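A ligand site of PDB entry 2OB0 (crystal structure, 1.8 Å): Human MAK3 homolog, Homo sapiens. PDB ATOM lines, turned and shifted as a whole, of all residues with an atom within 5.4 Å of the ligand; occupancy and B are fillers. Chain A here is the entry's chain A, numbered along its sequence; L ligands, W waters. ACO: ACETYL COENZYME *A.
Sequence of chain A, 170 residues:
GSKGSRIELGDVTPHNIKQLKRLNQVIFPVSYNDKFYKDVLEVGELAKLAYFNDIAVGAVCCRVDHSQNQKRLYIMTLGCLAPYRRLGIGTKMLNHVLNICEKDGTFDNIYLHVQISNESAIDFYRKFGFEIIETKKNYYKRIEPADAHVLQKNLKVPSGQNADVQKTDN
The backbone NH of Gly 88 lies within hydrogen-bond range of an oxygen (O1A) of the ligand, 2.9 Å away.
The backbone NH (N) of Thr 91 lies within hydrogen-bond range of an oxygen (O2A) of the ligand (2.9 Å).
The backbone NH (N) of Leu 87 sits at hydrogen-bond distance from an oxygen (O1A) of the ligand (3.3 Å).
NE of Arg 85 sits close to O9P of the ligand, 3.5 Å away.
O4A of the ligand is in hydrogen-bond range of N of Gly 90 (2.8 Å).
N of Cys 80 sits at hydrogen-bond distance from O9P of the ligand.
The backbone NH of Gln 115 is in hydrogen-bond range of an oxygen (O) of the ligand (3.0 Å).
NE of Arg 86 is in salt-bridge range of O9A of the ligand (2.7 Å).
An oxygen (O5P) of the ligand lies within hydrogen-bond range of the side-chain amide nitrogen of Asn 118 (2.8 Å).
An oxygen (O2A) of the ligand lies within hydrogen-bond range of the side-chain hydroxyl (OG1) of Thr 91, at 2.6 Å.
O4A of the ligand sits at hydrogen-bond distance from N of Ile 89, 3.5 Å away.
N of Arg 86 sits at hydrogen-bond distance from O5A of the ligand, 2.9 Å away.
Residues that only touch the ligand: Gly 79 (3.1 Å), Ser 120 (3.1 Å), Asp 123 (3.2 Å), Phe 124 (3.3 Å), Lys 127 (3.3 Å), Tyr 140 (3.4 Å), Pro 29 (3.5 Å), Phe 28 (3.6 Å), Leu 78 (3.7 Å), His 113 (3.7 Å), Val 114 (3.7 Å), Ala 121 (3.7 Å) and Ile 27 (3.9 Å).
Of the 30 residues printed, 23 come within 4 Å of the ligand.
The nearest printed residue that does not touch the ligand is Leu 112 (4.3 Å).
N of Ala 121 is in hydrogen-bond range of OD1 of Asn 118, at 3.1 Å.
OD1 of Asn 118 sits at hydrogen-bond distance from OG of Ser 120 (3.4 Å).
The backbone NH (N) of Gln 115 sits at hydrogen-bond distance from the side-chain hydroxyl (OH) of Tyr 140 (3.4 Å).
The backbone carbonyl oxygen (O) of Cys 80 sits at hydrogen-bond distance from the guanidinium group (NH2) of Arg 85 (2.9 Å).
Water W2 lies within hydrogen-bond range of O of Leu 78, OH of Tyr 125 and N4P of the ligand.
Water W1 bridges an oxygen (O5P) of the ligand (3.0 Å) and the backbone carbonyl oxygen of Ile 27 (3.0 Å).
Water W6 lies within hydrogen-bond range of the side-chain amide oxygen (OD1) of Asn 118 (2.7 Å), the side-chain hydroxyl (OG) of Ser 120 (2.8 Å) and a nitrogen (N8P) of the ligand (3.0 Å).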
ATOM      1  N   ILE A  27      29.862 -16.832   7.315  1.00  0.00           N
ATOM      2  CA  ILE A  27      29.428 -16.223   8.553  1.00  0.00           C
ATOM      3  C   ILE A  27      29.491 -17.155   9.771  1.00  0.00           C
ATOM      4  O   ILE A  27      29.838 -16.706  10.868  1.00  0.00           O
ATOM      5  CB  ILE A  27      28.007 -15.637   8.373  1.00  0.00           C
ATOM      6  CG1 ILE A  27      28.028 -14.525   7.315  1.00  0.00           C
ATOM      7  CG2 ILE A  27      27.469 -15.070   9.696  1.00  0.00           C
ATOM      8  CD1 ILE A  27      26.629 -14.119   6.810  1.00  0.00           C
ATOM      9  N   PHE A  28      29.158 -18.447   9.566  1.00  0.00           N
ATOM     10  CA  PHE A  28      29.031 -19.413  10.683  1.00  0.00           C
ATOM     11  C   PHE A  28      30.143 -20.450  10.679  1.00  0.00           C
ATOM     12  O   PHE A  28      30.561 -20.905   9.610  1.00  0.00           O
ATOM     13  CB  PHE A  28      27.647 -20.095  10.658  1.00  0.00           C
ATOM     14  CG  PHE A  28      26.511 -19.105  10.708  1.00  0.00           C
ATOM     15  CD1 PHE A  28      26.178 -18.490  11.905  1.00  0.00           C
ATOM     16  CD2 PHE A  28      25.819 -18.755   9.545  1.00  0.00           C
ATOM     17  CE1 PHE A  28      25.122 -17.560  11.957  1.00  0.00           C
ATOM     18  CE2 PHE A  28      24.810 -17.804   9.572  1.00  0.00           C
ATOM     19  CZ  PHE A  28      24.457 -17.200  10.815  1.00  0.00           C
ATOM     20  N   PRO A  29      30.636 -20.841  11.883  1.00  0.00           N
ATOM     21  CA  PRO A  29      31.793 -21.744  11.939  1.00  0.00           C
ATOM     22  C   PRO A  29      31.433 -23.223  11.748  1.00  0.00           C
ATOM     23  O   PRO A  29      32.328 -24.078  11.828  1.00  0.00           O
ATOM     24  CB  PRO A  29      32.312 -21.522  13.359  1.00  0.00           C
ATOM     25  CG  PRO A  29      31.052 -21.233  14.156  1.00  0.00           C
ATOM     26  CD  PRO A  29      30.183 -20.412  13.226  1.00  0.00           C
ATOM     27  N   LEU A  78      21.253 -16.805  12.087  1.00  0.00           N
ATOM     28  CA  LEU A  78      20.892 -15.390  11.861  1.00  0.00           C
ATOM     29  C   LEU A  78      22.187 -14.637  11.912  1.00  0.00           C
ATOM     30  O   LEU A  78      22.883 -14.657  12.935  1.00  0.00           O
ATOM     31  CB  LEU A  78      19.954 -14.889  12.949  1.00  0.00           C
ATOM     32  CG  LEU A  78      19.371 -13.455  12.901  1.00  0.00           C
ATOM     33  CD1 LEU A  78      18.120 -13.388  13.764  1.00  0.00           C
ATOM     34  CD2 LEU A  78      20.372 -12.326  13.346  1.00  0.00           C
ATOM     35  N   GLY A  79      22.569 -14.002  10.810  1.00  0.00           N
ATOM     36  CA  GLY A  79      23.828 -13.268  10.852  1.00  0.00           C
ATOM     37  C   GLY A  79      24.097 -12.517   9.570  1.00  0.00           C
ATOM     38  O   GLY A  79      23.394 -12.706   8.576  1.00  0.00           O
ATOM     39  N   CYS A  80      25.088 -11.638   9.608  1.00  0.00           N
ATOM     40  CA  CYS A  80      25.475 -10.945   8.393  1.00  0.00           C
ATOM     41  C   CYS A  80      26.989 -10.838   8.341  1.00  0.00           C
ATOM     42  O   CYS A  80      27.679 -11.086   9.318  1.00  0.00           O
ATOM     43  CB  CYS A  80      24.778  -9.585   8.248  1.00  0.00           C
ATOM     44  SG  CYS A  80      25.316  -8.257   9.386  1.00  0.00           S
ATOM     45  N   TYR A  84      29.413  -5.392   7.519  1.00  0.00           N
ATOM     46  CA  TYR A  84      28.093  -4.745   7.518  1.00  0.00           C
ATOM     47  C   TYR A  84      27.395  -4.809   8.890  1.00  0.00           C
ATOM     48  O   TYR A  84      26.219  -4.445   9.024  1.00  0.00           O
ATOM     49  CB  TYR A  84      27.201  -5.377   6.448  1.00  0.00           C
ATOM     50  CG  TYR A  84      27.744  -5.179   5.051  1.00  0.00           C
ATOM     51  CD1 TYR A  84      27.487  -4.002   4.359  1.00  0.00           C
ATOM     52  CD2 TYR A  84      28.526  -6.156   4.432  1.00  0.00           C
ATOM     53  CE1 TYR A  84      27.980  -3.805   3.062  1.00  0.00           C
ATOM     54  CE2 TYR A  84      29.055  -5.940   3.145  1.00  0.00           C
ATOM     55  CZ  TYR A  84      28.775  -4.767   2.491  1.00  0.00           C
ATOM     56  OH  TYR A  84      29.241  -4.516   1.229  1.00  0.00           O
ATOM     57  N   ARG A  85      28.155  -5.212   9.896  1.00  0.00           N
ATOM     58  CA  ARG A  85      27.605  -5.355  11.228  1.00  0.00           C
ATOM     59  C   ARG A  85      27.456  -3.992  11.883  1.00  0.00           C
ATOM     60  O   ARG A  85      28.102  -3.036  11.473  1.00  0.00           O
ATOM     61  CB  ARG A  85      28.447  -6.314  12.058  1.00  0.00           C
ATOM     62  CG  ARG A  85      28.132  -7.758  11.671  1.00  0.00           C
ATOM     63  CD  ARG A  85      28.952  -8.752  12.455  1.00  0.00           C
ATOM     64  NE  ARG A  85      28.983  -9.993  11.700  1.00  0.00           N
ATOM     65  CZ  ARG A  85      29.855 -10.968  11.879  1.00  0.00           C
ATOM     66  NH1 ARG A  85      30.751 -10.893  12.863  1.00  0.00           N
ATOM     67  NH2 ARG A  85      29.824 -12.026  11.072  1.00  0.00           N
ATOM     68  N   ARG A  86      26.580  -3.919  12.888  1.00  0.00           N
ATOM     69  CA  ARG A  86      26.218  -2.655  13.543  1.00  0.00           C
ATOM     70  C   ARG A  86      25.604  -1.602  12.642  1.00  0.00           C
ATOM     71  O   ARG A  86      25.840  -0.386  12.840  1.00  0.00           O
ATOM     72  CB  ARG A  86      27.386  -2.026  14.315  1.00  0.00           C
ATOM     73  CG  ARG A  86      27.876  -2.791  15.536  1.00  0.00           C
ATOM     74  CD  ARG A  86      26.796  -3.039  16.606  1.00  0.00           C
ATOM     75  NE  ARG A  86      26.556  -1.996  17.621  1.00  0.00           N
ATOM     76  CZ  ARG A  86      27.350  -1.737  18.663  1.00  0.00           C
ATOM     77  NH1 ARG A  86      28.512  -2.367  18.802  1.00  0.00           N
ATOM     78  NH2 ARG A  86      27.010  -0.827  19.553  1.00  0.00           N
ATOM     79  N   LEU A  87      24.811  -2.049  11.670  1.00  0.00           N
ATOM     80  CA  LEU A  87      24.045  -1.155  10.783  1.00  0.00           C
ATOM     81  C   LEU A  87      22.559  -1.442  10.895  1.00  0.00           C
ATOM     82  O   LEU A  87      21.753  -0.865  10.166  1.00  0.00           O
ATOM     83  CB  LEU A  87      24.452  -1.352   9.319  1.00  0.00           C
ATOM     84  CG  LEU A  87      25.907  -0.932   9.006  1.00  0.00           C
ATOM     85  CD1 LEU A  87      26.260  -1.295   7.564  1.00  0.00           C
ATOM     86  CD2 LEU A  87      26.113   0.546   9.244  1.00  0.00           C
ATOM     87  N   GLY A  88      22.186  -2.334  11.818  1.00  0.00           N
ATOM     88  CA  GLY A  88      20.773  -2.633  12.064  1.00  0.00           C
ATOM     89  C   GLY A  88      20.246  -3.798  11.260  1.00  0.00           C
ATOM     90  O   GLY A  88      19.050  -4.060  11.249  1.00  0.00           O
ATOM     91  N   ILE A  89      21.136  -4.539  10.589  1.00  0.00           N
ATOM     92  CA  ILE A  89      20.660  -5.657   9.795  1.00  0.00           C
ATOM     93  C   ILE A  89      20.138  -6.820  10.648  1.00  0.00           C
ATOM     94  O   ILE A  89      19.064  -7.361  10.384  1.00  0.00           O
ATOM     95  CB  ILE A  89      21.760  -6.157   8.856  1.00  0.00           C
ATOM     96  CG1 ILE A  89      22.076  -5.054   7.858  1.00  0.00           C
ATOM     97  CG2 ILE A  89      21.262  -7.415   8.129  1.00  0.00           C
ATOM     98  CD1 ILE A  89      23.331  -5.296   7.017  1.00  0.00           C
ATOM     99  N   GLY A  90      20.918  -7.190  11.669  1.00  0.00           N
ATOM    100  CA  GLY A  90      20.472  -8.163  12.668  1.00  0.00           C
ATOM    101  C   GLY A  90      19.121  -7.808  13.244  1.00  0.00           C
ATOM    102  O   GLY A  90      18.255  -8.664  13.353  1.00  0.00           O
ATOM    103  N   THR A  91      18.961  -6.544  13.678  1.00  0.00           N
ATOM    104  CA  THR A  91      17.706  -6.061  14.233  1.00  0.00           C
ATOM    105  C   THR A  91      16.563  -6.274  13.251  1.00  0.00           C
ATOM    106  O   THR A  91      15.472  -6.712  13.634  1.00  0.00           O
ATOM    107  CB  THR A  91      17.841  -4.586  14.640  1.00  0.00           C
ATOM    108  OG1 THR A  91      18.793  -4.490  15.709  1.00  0.00           O
ATOM    109  CG2 THR A  91      16.493  -3.997  15.082  1.00  0.00           C
ATOM    110  N   LYS A  92      16.804  -6.010  11.977  1.00  0.00           N
ATOM    111  CA  LYS A  92      15.742  -6.152  10.977  1.00  0.00           C
ATOM    112  C   LYS A  92      15.338  -7.639  10.851  1.00  0.00           C
ATOM    113  O   LYS A  92      14.148  -7.959  10.787  1.00  0.00           O
ATOM    114  CB  LYS A  92      16.239  -5.625   9.628  1.00  0.00           C
ATOM    115  CG  LYS A  92      15.206  -5.643   8.501  1.00  0.00           C
ATOM    116  CD  LYS A  92      14.665  -4.248   8.279  1.00  0.00           C
ATOM    117  CE  LYS A  92      13.835  -4.126   7.004  1.00  0.00           C
ATOM    118  NZ  LYS A  92      13.744  -2.677   6.645  1.00  0.00           N
ATOM    119  N   MET A  93      16.318  -8.528  10.837  1.00  0.00           N
ATOM    120  CA  MET A  93      16.046  -9.962  10.733  1.00  0.00           C
ATOM    121  C   MET A  93      15.360 -10.500  11.999  1.00  0.00           C
ATOM    122  O   MET A  93      14.390 -11.293  11.935  1.00  0.00           O
ATOM    123  CB  MET A  93      17.351 -10.724  10.444  1.00  0.00           C
ATOM    124  CG  MET A  93      17.957 -10.359   9.122  1.00  0.00           C
ATOM    125  SD  MET A  93      19.523 -11.499   8.760  1.00  0.00           S
ATOM    126  CE  MET A  93      20.803 -10.688   9.951  1.00  0.00           C
ATOM    127  N   LEU A 112      17.975 -19.981  20.683  1.00  0.00           N
ATOM    128  CA  LEU A 112      19.093 -20.365  19.847  1.00  0.00           C
ATOM    129  C   LEU A 112      20.289 -20.717  20.720  1.00  0.00           C
ATOM    130  O   LEU A 112      20.259 -20.517  21.932  1.00  0.00           O
ATOM    131  CB  LEU A 112      19.470 -19.226  18.915  1.00  0.00           C
ATOM    132  CG  LEU A 112      20.235 -18.042  19.506  1.00  0.00           C
ATOM    133  CD1 LEU A 112      21.069 -17.433  18.384  1.00  0.00           C
ATOM    134  CD2 LEU A 112      19.262 -17.013  20.067  1.00  0.00           C
ATOM    135  N   HIS A 113      21.336 -21.241  20.095  1.00  0.00           N
ATOM    136  CA  HIS A 113      22.618 -21.512  20.771  1.00  0.00           C
ATOM    137  C   HIS A 113      23.648 -20.498  20.308  1.00  0.00           C
ATOM    138  O   HIS A 113      23.746 -20.179  19.092  1.00  0.00           O
ATOM    139  CB  HIS A 113      23.115 -22.919  20.404  1.00  0.00           C
ATOM    140  CG  HIS A 113      22.204 -24.001  20.881  1.00  0.00           C
ATOM    141  ND1 HIS A 113      21.328 -24.655  20.057  1.00  0.00           N
ATOM    142  CD2 HIS A 113      22.006 -24.514  22.121  1.00  0.00           C
ATOM    143  CE1 HIS A 113      20.630 -25.540  20.747  1.00  0.00           C
ATOM    144  NE2 HIS A 113      21.021 -25.473  22.012  1.00  0.00           N
ATOM    145  N   VAL A 114      24.471 -20.039  21.243  1.00  0.00           N
ATOM    146  CA  VAL A 114      25.518 -19.037  20.948  1.00  0.00           C
ATOM    147  C   VAL A 114      26.802 -19.560  21.582  1.00  0.00           C
ATOM    148  O   VAL A 114      26.837 -19.815  22.786  1.00  0.00           O
ATOM    149  CB  VAL A 114      25.175 -17.636  21.550  1.00  0.00           C
ATOM    150  CG1 VAL A 114      26.315 -16.656  21.367  1.00  0.00           C
ATOM    151  CG2 VAL A 114      23.907 -17.043  20.865  1.00  0.00           C
ATOM    152  N   GLN A 115      27.855 -19.718  20.787  1.00  0.00           N
ATOM    153  CA  GLN A 115      29.144 -20.120  21.333  1.00  0.00           C
ATOM    154  C   GLN A 115      29.550 -19.161  22.438  1.00  0.00           C
ATOM    155  O   GLN A 115      29.433 -17.939  22.262  1.00  0.00           O
ATOM    156  CB  GLN A 115      30.179 -20.017  20.239  1.00  0.00           C
ATOM    157  CG  GLN A 115      31.443 -20.798  20.521  1.00  0.00           C
ATOM    158  CD  GLN A 115      32.339 -20.850  19.305  1.00  0.00           C
ATOM    159  OE1 GLN A 115      32.173 -20.061  18.359  1.00  0.00           O
ATOM    160  NE2 GLN A 115      33.301 -21.758  19.315  1.00  0.00           N
ATOM    161  N   ASN A 118      31.268 -15.723  21.949  1.00  0.00           N
ATOM    162  CA  ASN A 118      30.642 -14.790  21.025  1.00  0.00           C
ATOM    163  C   ASN A 118      30.001 -13.634  21.770  1.00  0.00           C
ATOM    164  O   ASN A 118      28.773 -13.570  21.911  1.00  0.00           O
ATOM    165  CB  ASN A 118      29.571 -15.513  20.187  1.00  0.00           C
ATOM    166  CG  ASN A 118      29.195 -14.749  18.912  1.00  0.00           C
ATOM    167  OD1 ASN A 118      29.289 -13.514  18.837  1.00  0.00           O
ATOM    168  ND2 ASN A 118      28.755 -15.502  17.902  1.00  0.00           N
ATOM    169  N   SER A 120      29.551 -10.494  21.043  1.00  0.00           N
ATOM    170  CA  SER A 120      28.674  -9.572  20.345  1.00  0.00           C
ATOM    171  C   SER A 120      27.280 -10.163  20.146  1.00  0.00           C
ATOM    172  O   SER A 120      26.295  -9.427  20.221  1.00  0.00           O
ATOM    173  CB  SER A 120      29.259  -9.105  19.022  1.00  0.00           C
ATOM    174  OG  SER A 120      29.419 -10.194  18.161  1.00  0.00           O
ATOM    175  N   ALA A 121      27.189 -11.481  19.946  1.00  0.00           N
ATOM    176  CA  ALA A 121      25.881 -12.122  19.795  1.00  0.00           C
ATOM    177  C   ALA A 121      25.171 -12.137  21.131  1.00  0.00           C
ATOM    178  O   ALA A 121      23.967 -11.952  21.172  1.00  0.00           O
ATOM    179  CB  ALA A 121      25.987 -13.512  19.259  1.00  0.00           C
ATOM    180  N   ASP A 123      25.454  -9.926  23.530  1.00  0.00           N
ATOM    181  CA  ASP A 123      24.979  -8.529  23.732  1.00  0.00           C
ATOM    182  C   ASP A 123      23.732  -8.263  22.887  1.00  0.00           C
ATOM    183  O   ASP A 123      22.765  -7.662  23.341  1.00  0.00           O
ATOM    184  CB  ASP A 123      26.043  -7.541  23.256  1.00  0.00           C
ATOM    185  CG  ASP A 123      27.208  -7.410  24.213  1.00  0.00           C
ATOM    186  OD1 ASP A 123      26.982  -7.574  25.434  1.00  0.00           O
ATOM    187  OD2 ASP A 123      28.343  -7.084  23.753  1.00  0.00           O
ATOM    188  N   PHE A 124      23.784  -8.693  21.640  1.00  0.00           N
ATOM    189  CA  PHE A 124      22.691  -8.438  20.694  1.00  0.00           C
ATOM    190  C   PHE A 124      21.404  -9.103  21.175  1.00  0.00           C
ATOM    191  O   PHE A 124      20.371  -8.452  21.264  1.00  0.00           O
ATOM    192  CB  PHE A 124      23.104  -9.019  19.334  1.00  0.00           C
ATOM    193  CG  PHE A 124      22.000  -9.029  18.299  1.00  0.00           C
ATOM    194  CD1 PHE A 124      21.583  -7.828  17.679  1.00  0.00           C
ATOM    195  CD2 PHE A 124      21.374 -10.236  17.952  1.00  0.00           C
ATOM    196  CE1 PHE A 124      20.573  -7.840  16.688  1.00  0.00           C
ATOM    197  CE2 PHE A 124      20.339 -10.244  16.979  1.00  0.00           C
ATOM    198  CZ  PHE A 124      19.950  -9.066  16.352  1.00  0.00           C
ATOM    199  N   TYR A 125      21.436 -10.385  21.480  1.00  0.00           N
ATOM    200  CA  TYR A 125      20.187 -11.071  21.875  1.00  0.00           C
ATOM    201  C   TYR A 125      19.690 -10.606  23.231  1.00  0.00           C
ATOM    202  O   TYR A 125      18.469 -10.491  23.454  1.00  0.00           O
ATOM    203  CB  TYR A 125      20.392 -12.578  21.873  1.00  0.00           C
ATOM    204  CG  TYR A 125      20.390 -13.112  20.454  1.00  0.00           C
ATOM    205  CD1 TYR A 125      19.193 -13.182  19.742  1.00  0.00           C
ATOM    206  CD2 TYR A 125      21.557 -13.493  19.822  1.00  0.00           C
ATOM    207  CE1 TYR A 125      19.149 -13.667  18.376  1.00  0.00           C
ATOM    208  CE2 TYR A 125      21.534 -13.943  18.458  1.00  0.00           C
ATOM    209  CZ  TYR A 125      20.330 -14.041  17.769  1.00  0.00           C
ATOM    210  OH  TYR A 125      20.312 -14.508  16.446  1.00  0.00           O
ATOM    211  N   LYS A 127      19.815  -7.707  24.320  1.00  0.00           N
ATOM    212  CA  LYS A 127      19.145  -6.435  24.070  1.00  0.00           C
ATOM    213  C   LYS A 127      17.656  -6.634  23.769  1.00  0.00           C
ATOM    214  O   LYS A 127      16.841  -5.803  24.112  1.00  0.00           O
ATOM    215  CB  LYS A 127      19.814  -5.682  22.911  1.00  0.00           C
ATOM    216  CG  LYS A 127      19.334  -4.240  22.764  1.00  0.00           C
ATOM    217  CD  LYS A 127      19.920  -3.580  21.531  1.00  0.00           C
ATOM    218  CE  LYS A 127      19.498  -2.106  21.378  1.00  0.00           C
ATOM    219  NZ  LYS A 127      19.949  -1.222  22.506  1.00  0.00           N
ATOM    220  N   PHE A 128      17.310  -7.744  23.106  1.00  0.00           N
ATOM    221  CA  PHE A 128      15.923  -8.021  22.721  1.00  0.00           C
ATOM    222  C   PHE A 128      15.163  -8.834  23.754  1.00  0.00           C
ATOM    223  O   PHE A 128      14.069  -9.334  23.465  1.00  0.00           O
ATOM    224  CB  PHE A 128      15.869  -8.740  21.379  1.00  0.00           C
ATOM    225  CG  PHE A 128      16.242  -7.871  20.220  1.00  0.00           C
ATOM    226  CD1 PHE A 128      15.245  -7.307  19.422  1.00  0.00           C
ATOM    227  CD2 PHE A 128      17.567  -7.618  19.931  1.00  0.00           C
ATOM    228  CE1 PHE A 128      15.587  -6.504  18.341  1.00  0.00           C
ATOM    229  CE2 PHE A 128      17.930  -6.802  18.877  1.00  0.00           C
ATOM    230  CZ  PHE A 128      16.944  -6.247  18.079  1.00  0.00           C
ATOM    231  N   TYR A 140      29.552 -27.996  20.473  1.00  0.00           N
ATOM    232  CA  TYR A 140      30.228 -28.114  19.175  1.00  0.00           C
ATOM    233  C   TYR A 140      31.231 -29.250  19.225  1.00  0.00           C
ATOM    234  O   TYR A 140      31.836 -29.509  20.259  1.00  0.00           O
ATOM    235  CB  TYR A 140      30.932 -26.818  18.788  1.00  0.00           C
ATOM    236  CG  TYR A 140      30.010 -25.622  18.754  1.00  0.00           C
ATOM    237  CD1 TYR A 140      29.155 -25.399  17.667  1.00  0.00           C
ATOM    238  CD2 TYR A 140      29.983 -24.701  19.812  1.00  0.00           C
ATOM    239  CE1 TYR A 140      28.292 -24.297  17.634  1.00  0.00           C
ATOM    240  CE2 TYR A 140      29.149 -23.598  19.776  1.00  0.00           C
ATOM    241  CZ  TYR A 140      28.296 -23.404  18.692  1.00  0.00           C
ATOM    242  OH  TYR A 140      27.452 -22.302  18.691  1.00  0.00           O
ATOM    243  N   ILE A 143      34.941 -27.127  16.918  1.00  0.00           N
ATOM    244  CA  ILE A 143      35.429 -25.759  17.095  1.00  0.00           C
ATOM    245  C   ILE A 143      35.621 -25.456  18.578  1.00  0.00           C
ATOM    246  O   ILE A 143      35.030 -26.125  19.416  1.00  0.00           O
ATOM    247  CB  ILE A 143      34.486 -24.689  16.420  1.00  0.00           C
ATOM    248  CG1 ILE A 143      33.134 -24.661  17.123  1.00  0.00           C
ATOM    249  CG2 ILE A 143      34.354 -24.956  14.916  1.00  0.00           C
ATOM    250  CD1 ILE A 143      32.201 -23.526  16.655  1.00  0.00           C
HETATM  251  N1A ACO L   1      28.996  -5.129  20.825  1.00  0.00           N
HETATM  252  C2A ACO L   1      28.045  -4.665  21.672  1.00  0.00           C
HETATM  253  N3A ACO L   1      26.733  -4.636  21.372  1.00  0.00           N
HETATM  254  C4A ACO L   1      26.295  -5.093  20.165  1.00  0.00           C
HETATM  255  C5A ACO L   1      27.279  -5.616  19.190  1.00  0.00           C
HETATM  256  C6A ACO L   1      28.704  -5.614  19.593  1.00  0.00           C
HETATM  257  N6A ACO L   1      29.676  -6.064  18.773  1.00  0.00           N
HETATM  258  N7A ACO L   1      26.577  -5.995  18.092  1.00  0.00           N
HETATM  259  C8A ACO L   1      25.278  -5.713  18.359  1.00  0.00           C
HETATM  260  N9A ACO L   1      25.101  -5.178  19.582  1.00  0.00           N
HETATM  261  C1B ACO L   1      23.799  -4.770  20.160  1.00  0.00           C
HETATM  262  C2B ACO L   1      23.709  -3.251  20.278  1.00  0.00           C
HETATM  263  O2B ACO L   1      23.215  -2.994  21.585  1.00  0.00           O
HETATM  264  C3B ACO L   1      22.529  -2.773  19.443  1.00  0.00           C
HETATM  265  O3B ACO L   1      22.702  -1.767  18.464  1.00  0.00           O
HETATM  266  P3B ACO L   1      23.417  -0.326  18.552  1.00  0.00           P
HETATM  267  O7A ACO L   1      22.240   0.606  18.419  1.00  0.00           O
HETATM  268  O8A ACO L   1      24.143  -0.278  19.889  1.00  0.00           O
HETATM  269  O9A ACO L   1      24.327  -0.448  17.342  1.00  0.00           O
HETATM  270  C4B ACO L   1      21.946  -4.041  18.817  1.00  0.00           C
HETATM  271  O4B ACO L   1      22.779  -5.131  19.210  1.00  0.00           O
HETATM  272  C5B ACO L   1      21.636  -3.967  17.306  1.00  0.00           C
HETATM  273  O5B ACO L   1      22.728  -4.401  16.486  1.00  0.00           O
HETATM  274  P1A ACO L   1      22.532  -4.582  14.893  1.00  0.00           P
HETATM  275  O1A ACO L   1      23.378  -3.628  14.129  1.00  0.00           O
HETATM  276  O2A ACO L   1      21.082  -4.759  14.587  1.00  0.00           O
HETATM  277  O3A ACO L   1      23.183  -6.037  14.854  1.00  0.00           O
HETATM  278  P2A ACO L   1      24.073  -6.719  13.684  1.00  0.00           P
HETATM  279  O4A ACO L   1      23.502  -6.427  12.313  1.00  0.00           O
HETATM  280  O5A ACO L   1      25.504  -6.395  13.881  1.00  0.00           O
HETATM  281  O6A ACO L   1      23.905  -8.266  14.000  1.00  0.00           O
HETATM  282  CBP ACO L   1      24.745 -10.294  14.991  1.00  0.00           C
HETATM  283  CCP ACO L   1      24.265  -8.857  15.258  1.00  0.00           C
HETATM  284  CDP ACO L   1      23.691 -11.030  14.147  1.00  0.00           C
HETATM  285  CEP ACO L   1      24.893 -11.046  16.312  1.00  0.00           C
HETATM  286  CAP ACO L   1      26.067 -10.175  14.214  1.00  0.00           C
HETATM  287  OAP ACO L   1      27.216  -9.894  15.048  1.00  0.00           O
HETATM  288  C9P ACO L   1      26.406 -11.424  13.442  1.00  0.00           C
HETATM  289  O9P ACO L   1      25.935 -11.577  12.324  1.00  0.00           O
HETATM  290  N8P ACO L   1      27.202 -12.308  14.030  1.00  0.00           N
HETATM  291  C7P ACO L   1      27.603 -13.562  13.361  1.00  0.00           C
HETATM  292  C6P ACO L   1      26.536 -14.651  13.464  1.00  0.00           C
HETATM  293  C5P ACO L   1      26.545 -15.209  14.875  1.00  0.00           C
HETATM  294  O5P ACO L   1      27.620 -15.467  15.396  1.00  0.00           O
HETATM  295  N4P ACO L   1      25.400 -15.492  15.493  1.00  0.00           N
HETATM  296  C3P ACO L   1      25.387 -16.234  16.760  1.00  0.00           C
HETATM  297  C2P ACO L   1      25.005 -17.716  16.682  1.00  0.00           C
HETATM  298  S1P ACO L   1      26.226 -18.662  15.811  1.00  0.00           S
HETATM  299  C   ACO L   1      27.508 -19.120  16.818  1.00  0.00           C
HETATM  300  O   ACO L   1      27.650 -18.664  17.955  1.00  0.00           O
HETATM  301  CH3 ACO L   1      28.472 -20.125  16.295  1.00  0.00           C
HETATM  302  O   HOH W   1      29.569 -17.133  13.853  1.00  0.00           O
HETATM  303  O   HOH W   2      22.610 -15.538  15.350  1.00  0.00           O
HETATM  304  O   HOH W   3      22.855  -1.070  15.128  1.00  0.00           O
HETATM  305  O   HOH W   4      24.942  -3.401  23.492  1.00  0.00           O
HETATM  306  O   HOH W   5      24.079  -4.607  10.657  1.00  0.00           O
HETATM  307  O   HOH W   6      28.993 -12.292  16.433  1.00  0.00           O
HETATM  308  O   HOH W   7      27.267  -7.072  15.669  1.00  0.00           O
HETATM  309  O   HOH W   8      18.487  -2.861  17.996  1.00  0.00           O
HETATM  310  O   HOH W   9      29.907  -6.611  15.618  1.00  0.00           O
HETATM  311  O   HOH W  10      22.107 -18.090  14.854  1.00  0.00           O
